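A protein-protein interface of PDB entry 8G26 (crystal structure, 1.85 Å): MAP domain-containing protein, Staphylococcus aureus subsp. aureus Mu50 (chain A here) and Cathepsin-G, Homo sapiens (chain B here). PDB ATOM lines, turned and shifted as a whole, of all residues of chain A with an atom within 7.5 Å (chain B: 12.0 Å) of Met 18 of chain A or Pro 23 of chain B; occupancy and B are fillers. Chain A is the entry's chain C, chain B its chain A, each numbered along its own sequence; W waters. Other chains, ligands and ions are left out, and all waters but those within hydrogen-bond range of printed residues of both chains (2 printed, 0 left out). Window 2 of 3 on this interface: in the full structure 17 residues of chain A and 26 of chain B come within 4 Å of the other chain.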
ATOM      1  N   ALA A  15     -11.702 -32.720 -19.746  1.00  0.00           N
ATOM      2  CA  ALA A  15     -11.896 -32.536 -21.179  1.00  0.00           C
ATOM      3  C   ALA A  15     -12.088 -31.059 -21.528  1.00  0.00           C
ATOM      4  O   ALA A  15     -12.495 -30.727 -22.640  1.00  0.00           O
ATOM      5  CB  ALA A  15     -13.090 -33.353 -21.659  1.00  0.00           C
ATOM      6  N   LYS A  16     -11.798 -30.179 -20.572  1.00  0.00           N
ATOM      7  CA  LYS A  16     -11.916 -28.741 -20.784  1.00  0.00           C
ATOM      8  C   LYS A  16     -11.057 -28.021 -19.754  1.00  0.00           C
ATOM      9  O   LYS A  16     -10.769 -28.550 -18.679  1.00  0.00           O
ATOM     10  CB  LYS A  16     -13.378 -28.278 -20.708  1.00  0.00           C
ATOM     11  CG  LYS A  16     -14.156 -28.789 -19.499  1.00  0.00           C
ATOM     12  CD  LYS A  16     -15.613 -29.073 -19.860  1.00  0.00           C
ATOM     13  CE  LYS A  16     -15.746 -30.345 -20.688  1.00  0.00           C
ATOM     14  NZ  LYS A  16     -15.358 -31.550 -19.901  1.00  0.00           N
ATOM     15  N   GLU A  17     -10.654 -26.800 -20.102  1.00  0.00           N
ATOM     16  CA  GLU A  17      -9.707 -26.049 -19.288  1.00  0.00           C
ATOM     17  C   GLU A  17     -10.324 -25.649 -17.951  1.00  0.00           C
ATOM     18  O   GLU A  17     -11.542 -25.497 -17.821  1.00  0.00           O
ATOM     19  CB  GLU A  17      -9.234 -24.804 -20.046  1.00  0.00           C
ATOM     20  CG  GLU A  17     -10.355 -23.840 -20.440  1.00  0.00           C
ATOM     21  CD  GLU A  17     -10.431 -23.579 -21.943  1.00  0.00           C
ATOM     22  OE1 GLU A  17      -9.829 -24.349 -22.727  1.00  0.00           O
ATOM     23  OE2 GLU A  17     -11.098 -22.598 -22.344  1.00  0.00           O
ATOM     24  N   MET A  18      -9.459 -25.479 -16.945  1.00  0.00           N
ATOM     25  CA  MET A  18      -9.881 -25.114 -15.598  1.00  0.00           C
ATOM     26  C   MET A  18      -9.015 -23.983 -15.046  1.00  0.00           C
ATOM     27  O   MET A  18      -7.812 -23.916 -15.307  1.00  0.00           O
ATOM     28  CB  MET A  18      -9.825 -26.337 -14.650  1.00  0.00           C
ATOM     29  CG  MET A  18     -10.704 -27.527 -15.069  1.00  0.00           C
ATOM     30  SD  MET A  18     -12.233 -27.683 -14.110  1.00  0.00           S
ATOM     31  CE  MET A  18     -11.900 -29.113 -13.077  1.00  0.00           C
ATOM     32  N   GLN A  19      -9.670 -23.081 -14.315  1.00  0.00           N
ATOM     33  CA  GLN A  19      -9.038 -22.044 -13.512  1.00  0.00           C
ATOM     34  C   GLN A  19      -8.656 -22.598 -12.146  1.00  0.00           C
ATOM     35  O   GLN A  19      -9.420 -23.350 -11.536  1.00  0.00           O
ATOM     36  CB  GLN A  19     -10.026 -20.884 -13.350  1.00  0.00           C
ATOM     37  CG  GLN A  19      -9.546 -19.719 -12.515  1.00  0.00           C
ATOM     38  CD  GLN A  19      -8.457 -18.932 -13.208  1.00  0.00           C
ATOM     39  OE1 GLN A  19      -8.735 -18.062 -14.041  1.00  0.00           O
ATOM     40  NE2 GLN A  19      -7.202 -19.238 -12.874  1.00  0.00           N
ATOM     41  N   ASN A  20      -7.487 -22.197 -11.646  1.00  0.00           N
ATOM     42  CA  ASN A  20      -6.955 -22.703 -10.375  1.00  0.00           C
ATOM     43  C   ASN A  20      -6.958 -21.579  -9.346  1.00  0.00           C
ATOM     44  O   ASN A  20      -6.092 -20.704  -9.372  1.00  0.00           O
ATOM     45  CB  ASN A  20      -5.542 -23.254 -10.564  1.00  0.00           C
ATOM     46  CG  ASN A  20      -5.389 -24.029 -11.845  1.00  0.00           C
ATOM     47  OD1 ASN A  20      -4.516 -23.738 -12.663  1.00  0.00           O
ATOM     48  ND2 ASN A  20      -6.251 -25.016 -12.043  1.00  0.00           N
ATOM     49  N   VAL A  21      -7.910 -21.625  -8.423  1.00  0.00           N
ATOM     50  CA  VAL A  21      -8.127 -20.560  -7.450  1.00  0.00           C
ATOM     51  C   VAL A  21      -7.457 -20.973  -6.145  1.00  0.00           C
ATOM     52  O   VAL A  21      -7.835 -22.000  -5.580  1.00  0.00           O
ATOM     53  CB  VAL A  21      -9.627 -20.305  -7.225  1.00  0.00           C
ATOM     54  CG1 VAL A  21      -9.832 -19.174  -6.221  1.00  0.00           C
ATOM     55  CG2 VAL A  21     -10.335 -19.999  -8.547  1.00  0.00           C
ATOM     56  N   LEU A  38      -8.347 -24.684  -5.952  1.00  0.00           N
ATOM     57  CA  LEU A  38      -9.638 -25.216  -6.351  1.00  0.00           C
ATOM     58  C   LEU A  38      -9.840 -25.025  -7.852  1.00  0.00           C
ATOM     59  O   LEU A  38      -9.640 -23.926  -8.375  1.00  0.00           O
ATOM     60  CB  LEU A  38     -10.753 -24.507  -5.573  1.00  0.00           C
ATOM     61  CG  LEU A  38     -12.161 -24.931  -5.976  1.00  0.00           C
ATOM     62  CD1 LEU A  38     -12.346 -26.395  -5.592  1.00  0.00           C
ATOM     63  CD2 LEU A  38     -13.218 -24.053  -5.350  1.00  0.00           C
ATOM     64  N   ASN A  39     -10.224 -26.099  -8.541  1.00  0.00           N
ATOM     65  CA  ASN A  39     -10.527 -26.004  -9.965  1.00  0.00           C
ATOM     66  C   ASN A  39     -11.931 -25.448 -10.175  1.00  0.00           C
ATOM     67  O   ASN A  39     -12.884 -25.871  -9.512  1.00  0.00           O
ATOM     68  CB  ASN A  39     -10.420 -27.364 -10.651  1.00  0.00           C
ATOM     69  CG  ASN A  39      -8.994 -27.763 -10.916  1.00  0.00           C
ATOM     70  OD1 ASN A  39      -8.107 -26.915 -10.978  1.00  0.00           O
ATOM     71  ND2 ASN A  39      -8.761 -29.066 -11.084  1.00  0.00           N
ATOM     72  N   LEU A  40     -12.049 -24.504 -11.091  1.00  0.00           N
ATOM     73  CA  LEU A  40     -13.328 -24.017 -11.576  1.00  0.00           C
ATOM     74  C   LEU A  40     -13.286 -24.077 -13.096  1.00  0.00           C
ATOM     75  O   LEU A  40     -12.259 -23.757 -13.684  1.00  0.00           O
ATOM     76  CB  LEU A  40     -13.592 -22.580 -11.132  1.00  0.00           C
ATOM     77  CG  LEU A  40     -13.670 -22.293  -9.635  1.00  0.00           C
ATOM     78  CD1 LEU A  40     -13.840 -20.796  -9.411  1.00  0.00           C
ATOM     79  CD2 LEU A  40     -14.810 -23.051  -9.027  1.00  0.00           C
ATOM     80  N   PRO A  41     -14.370 -24.448 -13.768  1.00  0.00           N
ATOM     81  CA  PRO A  41     -14.319 -24.479 -15.235  1.00  0.00           C
ATOM     82  C   PRO A  41     -14.044 -23.076 -15.763  1.00  0.00           C
ATOM     83  O   PRO A  41     -14.716 -22.113 -15.394  1.00  0.00           O
ATOM     84  CB  PRO A  41     -15.700 -24.999 -15.632  1.00  0.00           C
ATOM     85  CG  PRO A  41     -16.589 -24.635 -14.484  1.00  0.00           C
ATOM     86  CD  PRO A  41     -15.747 -24.530 -13.246  1.00  0.00           C
ATOM     87  N   LYS A  42     -13.026 -22.960 -16.609  1.00  0.00           N
ATOM     88  CA  LYS A  42     -12.592 -21.644 -17.047  1.00  0.00           C
ATOM     89  C   LYS A  42     -13.642 -21.007 -17.946  1.00  0.00           C
ATOM     90  O   LYS A  42     -14.378 -21.689 -18.663  1.00  0.00           O
ATOM     91  CB  LYS A  42     -11.262 -21.729 -17.795  1.00  0.00           C
ATOM     92  CG  LYS A  42     -10.603 -20.376 -18.048  1.00  0.00           C
ATOM     93  CD  LYS A  42      -9.189 -20.541 -18.586  1.00  0.00           C
ATOM     94  CE  LYS A  42      -8.129 -20.056 -17.593  1.00  0.00           C
ATOM     95  NZ  LYS A  42      -8.301 -20.628 -16.222  1.00  0.00           N
ATOM     96  N   ASP A  43     -13.703 -19.678 -17.905  1.00  0.00           N
ATOM     97  CA  ASP A  43     -14.606 -18.928 -18.769  1.00  0.00           C
ATOM     98  C   ASP A  43     -16.047 -19.371 -18.548  1.00  0.00           C
ATOM     99  O   ASP A  43     -16.851 -19.428 -19.483  1.00  0.00           O
ATOM    100  CB  ASP A  43     -14.202 -19.086 -20.238  1.00  0.00           C
ATOM    101  CG  ASP A  43     -12.773 -18.632 -20.504  1.00  0.00           C
ATOM    102  OD1 ASP A  43     -12.378 -17.563 -19.989  1.00  0.00           O
ATOM    103  OD2 ASP A  43     -12.039 -19.344 -21.228  1.00  0.00           O
ATOM    104  N   LYS A  54     -19.257 -26.454  -3.470  1.00  0.00           N
ATOM    105  CA  LYS A  54     -17.855 -26.834  -3.642  1.00  0.00           C
ATOM    106  C   LYS A  54     -17.053 -26.597  -2.370  1.00  0.00           C
ATOM    107  O   LYS A  54     -16.168 -27.396  -2.024  1.00  0.00           O
ATOM    108  CB  LYS A  54     -17.250 -26.043  -4.792  1.00  0.00           C
ATOM    109  CG  LYS A  54     -17.846 -26.435  -6.129  1.00  0.00           C
ATOM    110  CD  LYS A  54     -17.729 -25.318  -7.127  1.00  0.00           C
ATOM    111  CE  LYS A  54     -16.625 -25.614  -8.097  1.00  0.00           C
ATOM    112  NZ  LYS A  54     -15.331 -25.730  -7.363  1.00  0.00           N
ATOM    113  N   SER A 104     -16.221 -17.355 -13.258  1.00  0.00           N
ATOM    114  CA  SER A 104     -15.149 -18.089 -12.588  1.00  0.00           C
ATOM    115  C   SER A 104     -13.825 -17.337 -12.668  1.00  0.00           C
ATOM    116  O   SER A 104     -12.990 -17.449 -11.762  1.00  0.00           O
ATOM    117  CB  SER A 104     -14.999 -19.485 -13.197  1.00  0.00           C
ATOM    118  OG  SER A 104     -14.680 -19.422 -14.581  1.00  0.00           O
ATOM    119  N   ASN A 105     -13.626 -16.554 -13.729  1.00  0.00           N
ATOM    120  CA  ASN A 105     -12.368 -15.851 -13.945  1.00  0.00           C
ATOM    121  C   ASN A 105     -12.162 -14.671 -13.005  1.00  0.00           C
ATOM    122  O   ASN A 105     -11.079 -14.079 -13.019  1.00  0.00           O
ATOM    123  CB  ASN A 105     -12.296 -15.343 -15.388  1.00  0.00           C
ATOM    124  CG  ASN A 105     -12.498 -16.442 -16.401  1.00  0.00           C
ATOM    125  OD1 ASN A 105     -12.179 -17.605 -16.142  1.00  0.00           O
ATOM    126  ND2 ASN A 105     -13.030 -16.087 -17.563  1.00  0.00           N
ATOM    127  N   GLN B  19       4.190 -31.878  -6.605  1.00  0.00           N
ATOM    128  CA  GLN B  19       3.017 -31.345  -7.293  1.00  0.00           C
ATOM    129  C   GLN B  19       1.917 -32.391  -7.273  1.00  0.00           C
ATOM    130  O   GLN B  19       2.071 -33.471  -7.846  1.00  0.00           O
ATOM    131  CB  GLN B  19       3.353 -30.957  -8.729  1.00  0.00           C
ATOM    132  CG  GLN B  19       4.401 -29.886  -8.829  1.00  0.00           C
ATOM    133  CD  GLN B  19       4.938 -29.764 -10.224  1.00  0.00           C
ATOM    134  OE1 GLN B  19       4.388 -29.042 -11.046  1.00  0.00           O
ATOM    135  NE2 GLN B  19       6.004 -30.487 -10.505  1.00  0.00           N
ATOM    136  N   ILE B  20       0.803 -32.064  -6.627  1.00  0.00           N
ATOM    137  CA  ILE B  20      -0.285 -32.996  -6.383  1.00  0.00           C
ATOM    138  C   ILE B  20      -1.505 -32.538  -7.177  1.00  0.00           C
ATOM    139  O   ILE B  20      -1.875 -31.362  -7.142  1.00  0.00           O
ATOM    140  CB  ILE B  20      -0.597 -33.071  -4.877  1.00  0.00           C
ATOM    141  CG1 ILE B  20       0.647 -33.507  -4.091  1.00  0.00           C
ATOM    142  CG2 ILE B  20      -1.736 -33.994  -4.639  1.00  0.00           C
ATOM    143  CD1 ILE B  20       1.208 -32.385  -3.240  1.00  0.00           C
ATOM    144  N   GLN B  21      -2.120 -33.457  -7.890  1.00  0.00           N
ATOM    145  CA  GLN B  21      -3.249 -33.168  -8.761  1.00  0.00           C
ATOM    146  C   GLN B  21      -4.368 -34.160  -8.486  1.00  0.00           C
ATOM    147  O   GLN B  21      -4.128 -35.353  -8.328  1.00  0.00           O
ATOM    148  CB  GLN B  21      -2.797 -33.233 -10.245  1.00  0.00           C
ATOM    149  CG  GLN B  21      -1.583 -32.341 -10.544  1.00  0.00           C
ATOM    150  CD  GLN B  21      -0.455 -33.073 -11.287  1.00  0.00           C
ATOM    151  OE1 GLN B  21       0.463 -33.637 -10.665  1.00  0.00           O
ATOM    152  NE2 GLN B  21      -0.515 -33.058 -12.615  1.00  0.00           N
ATOM    153  N   SER B  22      -5.585 -33.644  -8.397  1.00  0.00           N
ATOM    154  CA  SER B  22      -6.825 -34.388  -8.216  1.00  0.00           C
ATOM    155  C   SER B  22      -7.875 -33.696  -9.088  1.00  0.00           C
ATOM    156  O   SER B  22      -7.721 -32.518  -9.424  1.00  0.00           O
ATOM    157  CB  SER B  22      -7.290 -34.409  -6.751  1.00  0.00           C
ATOM    158  OG  SER B  22      -6.312 -34.941  -5.860  1.00  0.00           O
ATOM    159  N   PRO B  23      -8.962 -34.396  -9.435  1.00  0.00           N
ATOM    160  CA  PRO B  23      -9.969 -33.757 -10.309  1.00  0.00           C
ATOM    161  C   PRO B  23     -10.452 -32.411  -9.804  1.00  0.00           C
ATOM    162  O   PRO B  23     -10.681 -31.497 -10.599  1.00  0.00           O
ATOM    163  CB  PRO B  23     -11.105 -34.789 -10.334  1.00  0.00           C
ATOM    164  CG  PRO B  23     -10.405 -36.093 -10.202  1.00  0.00           C
ATOM    165  CD  PRO B  23      -9.233 -35.831  -9.238  1.00  0.00           C
ATOM    166  N   ALA B  24     -10.604 -32.256  -8.495  1.00  0.00           N
ATOM    167  CA  ALA B  24     -11.166 -31.025  -7.961  1.00  0.00           C
ATOM    168  C   ALA B  24     -10.131 -29.936  -7.722  1.00  0.00           C
ATOM    169  O   ALA B  24     -10.521 -28.794  -7.461  1.00  0.00           O
ATOM    170  CB  ALA B  24     -11.906 -31.305  -6.646  1.00  0.00           C
ATOM    171  N   GLY B  25      -8.836 -30.233  -7.801  1.00  0.00           N
ATOM    172  CA  GLY B  25      -7.862 -29.216  -7.476  1.00  0.00           C
ATOM    173  C   GLY B  25      -6.446 -29.755  -7.473  1.00  0.00           C
ATOM    174  O   GLY B  25      -6.171 -30.848  -7.963  1.00  0.00           O
ATOM    175  N   GLN B  26      -5.557 -28.931  -6.923  1.00  0.00           N
ATOM    176  CA  GLN B  26      -4.134 -29.201  -6.889  1.00  0.00           C
ATOM    177  C   GLN B  26      -3.554 -28.706  -5.582  1.00  0.00           C
ATOM    178  O   GLN B  26      -4.138 -27.867  -4.898  1.00  0.00           O
ATOM    179  CB  GLN B  26      -3.356 -28.500  -8.000  1.00  0.00           C
ATOM    180  CG  GLN B  26      -3.507 -29.083  -9.331  1.00  0.00           C
ATOM    181  CD  GLN B  26      -3.925 -28.038 -10.301  1.00  0.00           C
ATOM    182  OE1 GLN B  26      -4.727 -27.168  -9.967  1.00  0.00           O
ATOM    183  NE2 GLN B  26      -3.366 -28.087 -11.507  1.00  0.00           N
ATOM    184  N   SER B  27      -2.378 -29.228  -5.263  1.00  0.00           N
ATOM    185  CA  SER B  27      -1.622 -28.768  -4.116  1.00  0.00           C
ATOM    186  C   SER B  27      -0.139 -28.851  -4.431  1.00  0.00           C
ATOM    187  O   SER B  27       0.297 -29.592  -5.311  1.00  0.00           O
ATOM    188  CB  SER B  27      -1.931 -29.591  -2.854  1.00  0.00           C
ATOM    189  OG  SER B  27      -3.328 -29.639  -2.629  1.00  0.00           O
ATOM    190  N   ARG B  28       0.630 -28.052  -3.706  1.00  0.00           N
ATOM    191  CA  ARG B  28       2.084 -28.078  -3.749  1.00  0.00           C
ATOM    192  C   ARG B  28       2.568 -28.310  -2.328  1.00  0.00           C
ATOM    193  O   ARG B  28       2.052 -27.698  -1.381  1.00  0.00           O
ATOM    194  CB  ARG B  28       2.655 -26.786  -4.326  1.00  0.00           C
ATOM    195  CG  ARG B  28       1.944 -26.281  -5.591  1.00  0.00           C
ATOM    196  CD  ARG B  28       2.485 -26.854  -6.902  1.00  0.00           C
ATOM    197  NE  ARG B  28       1.745 -28.021  -7.375  1.00  0.00           N
ATOM    198  CZ  ARG B  28       0.655 -27.979  -8.133  1.00  0.00           C
ATOM    199  NH1 ARG B  28       0.127 -26.827  -8.534  1.00  0.00           N
ATOM    200  NH2 ARG B  28       0.072 -29.122  -8.488  1.00  0.00           N
ATOM    201  N   CYS B  45      -1.016 -33.797   2.264  1.00  0.00           N
ATOM    202  CA  CYS B  45      -0.565 -33.525   0.902  1.00  0.00           C
ATOM    203  C   CYS B  45      -1.026 -34.592  -0.098  1.00  0.00           C
ATOM    204  O   CYS B  45      -0.711 -34.490  -1.288  1.00  0.00           O
ATOM    205  CB  CYS B  45       0.973 -33.416   0.892  1.00  0.00           C
ATOM    206  SG  CYS B  45       1.645 -32.043   1.886  1.00  0.00           S
ATOM    207  N   TRP B  46      -1.784 -35.591   0.352  1.00  0.00           N
ATOM    208  CA  TRP B  46      -2.171 -36.702  -0.511  1.00  0.00           C
ATOM    209  C   TRP B  46      -3.089 -36.219  -1.629  1.00  0.00           C
ATOM    210  O   TRP B  46      -3.789 -35.217  -1.503  1.00  0.00           O
ATOM    211  CB  TRP B  46      -2.841 -37.794   0.333  1.00  0.00           C
ATOM    212  CG  TRP B  46      -3.351 -38.963  -0.447  1.00  0.00           C
ATOM    213  CD1 TRP B  46      -2.676 -40.077  -0.775  1.00  0.00           C
ATOM    214  CD2 TRP B  46      -4.676 -39.113  -0.998  1.00  0.00           C
ATOM    215  NE1 TRP B  46      -3.479 -40.924  -1.502  1.00  0.00           N
ATOM    216  CE2 TRP B  46      -4.719 -40.351  -1.640  1.00  0.00           C
ATOM    217  CE3 TRP B  46      -5.831 -38.324  -0.969  1.00  0.00           C
ATOM    218  CZ2 TRP B  46      -5.860 -40.820  -2.286  1.00  0.00           C
ATOM    219  CZ3 TRP B  46      -6.962 -38.788  -1.620  1.00  0.00           C
ATOM    220  CH2 TRP B  46      -6.965 -40.017  -2.267  1.00  0.00           C
ATOM    221  N   GLY B  47      -3.028 -36.909  -2.760  1.00  0.00           N
ATOM    222  CA  GLY B  47      -3.910 -36.598  -3.873  1.00  0.00           C
ATOM    223  C   GLY B  47      -3.844 -37.720  -4.884  1.00  0.00           C
ATOM    224  O   GLY B  47      -3.126 -38.703  -4.700  1.00  0.00           O
ATOM    225  N   SER B  48      -4.603 -37.561  -5.974  1.00  0.00           N
ATOM    226  CA  SER B  48      -4.752 -38.673  -6.922  1.00  0.00           C
ATOM    227  C   SER B  48      -3.470 -38.954  -7.700  1.00  0.00           C
ATOM    228  O   SER B  48      -3.182 -40.113  -8.036  1.00  0.00           O
ATOM    229  CB  SER B  48      -5.872 -38.388  -7.925  1.00  0.00           C
ATOM    230  OG  SER B  48      -7.089 -38.082  -7.296  1.00  0.00           O
ATOM    231  N   ASN B  49      -2.728 -37.913  -8.057  1.00  0.00           N
ATOM    232  CA  ASN B  49      -1.470 -38.082  -8.782  1.00  0.00           C
ATOM    233  C   ASN B  49      -0.425 -37.159  -8.180  1.00  0.00           C
ATOM    234  O   ASN B  49      -0.727 -35.996  -7.898  1.00  0.00           O
ATOM    235  CB  ASN B  49      -1.658 -37.776 -10.274  1.00  0.00           C
ATOM    236  CG  ASN B  49      -2.668 -38.700 -10.929  1.00  0.00           C
ATOM    237  OD1 ASN B  49      -2.347 -39.836 -11.298  1.00  0.00           O
ATOM    238  ND2 ASN B  49      -3.897 -38.223 -11.074  1.00  0.00           N
ATOM    239  N   ILE B  50       0.776 -37.681  -7.943  1.00  0.00           N
ATOM    240  CA  ILE B  50       1.847 -36.927  -7.297  1.00  0.00           C
ATOM    241  C   ILE B  50       3.089 -37.008  -8.177  1.00  0.00           C
ATOM    242  O   ILE B  50       3.553 -38.105  -8.509  1.00  0.00           O
ATOM    243  CB  ILE B  50       2.143 -37.429  -5.873  1.00  0.00           C
ATOM    244  CG1 ILE B  50       0.856 -37.368  -5.042  1.00  0.00           C
ATOM    245  CG2 ILE B  50       3.207 -36.574  -5.220  1.00  0.00           C
ATOM    246  CD1 ILE B  50       1.015 -37.708  -3.572  1.00  0.00           C
HETATM  247  O   HOH W   1      -6.166 -31.026 -11.369  1.00  0.00           O
HETATM  248  O   HOH W   2     -13.394 -28.090  -8.355  1.00  0.00           O
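N of Gly 25 of chain B lies close to ND2 of Asn 39 of chain A, 3.5 Å away.
The side-chain amide nitrogen of Asn 39 of chain A is in hydrogen-bond range of the backbone carbonyl oxygen of Pro 23 of chain B (3.1 Å).
The backbone carbonyl oxygen of Ala 24 of chain B sits at hydrogen-bond distance from the backbone NH of Asn 39 of chain A.
OE1 of Gln 26 of chain B lies within hydrogen-bond range of ND2 of Asn 20 of chain A (3.4 Å).
Water W2 lies within hydrogen-bond range of the backbone carbonyl oxygen of Asn 39 of chain A (2.6 Å), the backbone carbonyl oxygen of Ala 24 of chain B (3.1 Å) and the side-chain amino group of Lys 54 of chain A (3.2 Å).
Water W1 lies within hydrogen-bond range of O of Ser 22 of chain B, ND2 of Asn 39 of chain A and O of Gly 25 of chain B.
O of Val 21 of chain A lies within hydrogen-bond range of N of Leu 38 of chain A (2.8 Å).
ND2 of Asn 20 of chain A lies within hydrogen-bond range of OD1 of Asn 39 of chain A, 2.9 Å away.
OG of Ser 22 of chain B is in hydrogen-bond range of N of Ser 48 of chain B (3.1 Å).
The backbone carbonyl oxygen of Met 18 of chain A sits at hydrogen-bond distance from the side-chain amino group of Lys 42 of chain A, at 3.4 Å.
The backbone carbonyl oxygen (O) of Asn 39 of chain A is in hydrogen-bond range of the side-chain amino group (NZ) of Lys 54 of chain A, at 3.3 Å.
No residue of chain B comes within 4 Å of Lys 16 of chain A.
Glu 17 of chain A touches none of the printed residues of chain B.
Met 18 of chain A touches one residue of chain B.
Gln 19 of chain A touches none of the printed residues of chain B.
Asn 20 of chain A touches just one residue of chain B: Gln 26 (3.4 Å).
No residue of chain B comes within 4 Å of Pro 41 of chain A.
No residue of chain B comes within 4 Å of Lys 42 of chain A.
Of the printed residues of chain A, Ser 22 of chain B touches Asn 39.
Pro 23 of chain B touches just these residues of chain A: Met 18 and Asn 39.
Of the printed residues of chain A, Ala 24 of chain B touches Leu 38 and Asn 39.
Of the printed residues of chain A, Gly 25 of chain B touches Asn 39 (3.5 Å).
Of the printed residues of chain A, Gln 26 of chain B touches Asn 20 (3.4 Å) and Asn 39 (3.5 Å).
The nearest residue of chain B that does not touch Met 18 of chain A is Ala 24 of chain B (5.5 Å).
Along chain B the printed residues that touch a printed residue of chain A span positions 22 to 26.
Printed residues of chain A that touch a printed residue of chain B: Met 18, Asn 20, Leu 38 and Asn 39.
Hydrophobic or aromatic side chains of chain A that line the printed part of chain B: Met 18 and Leu 38.
Among the printed residues, no Asp or Glu carboxylate lies within 4 Å of a Lys or Arg side-chain nitrogen of the other chain.
Met 18 of chain A touches Pro 23 of chain B (CE to O, 3.6 Å).
Leu 38 of chain A touches Ala 24 of chain B.
ND2 of Asn 39 of chain A touches O of Ser 22 of chain B, at 3.97 Å.
Gln 26 of chain B touches Asn 39 of chain A (OE1 to OD1, 3.5 Å).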
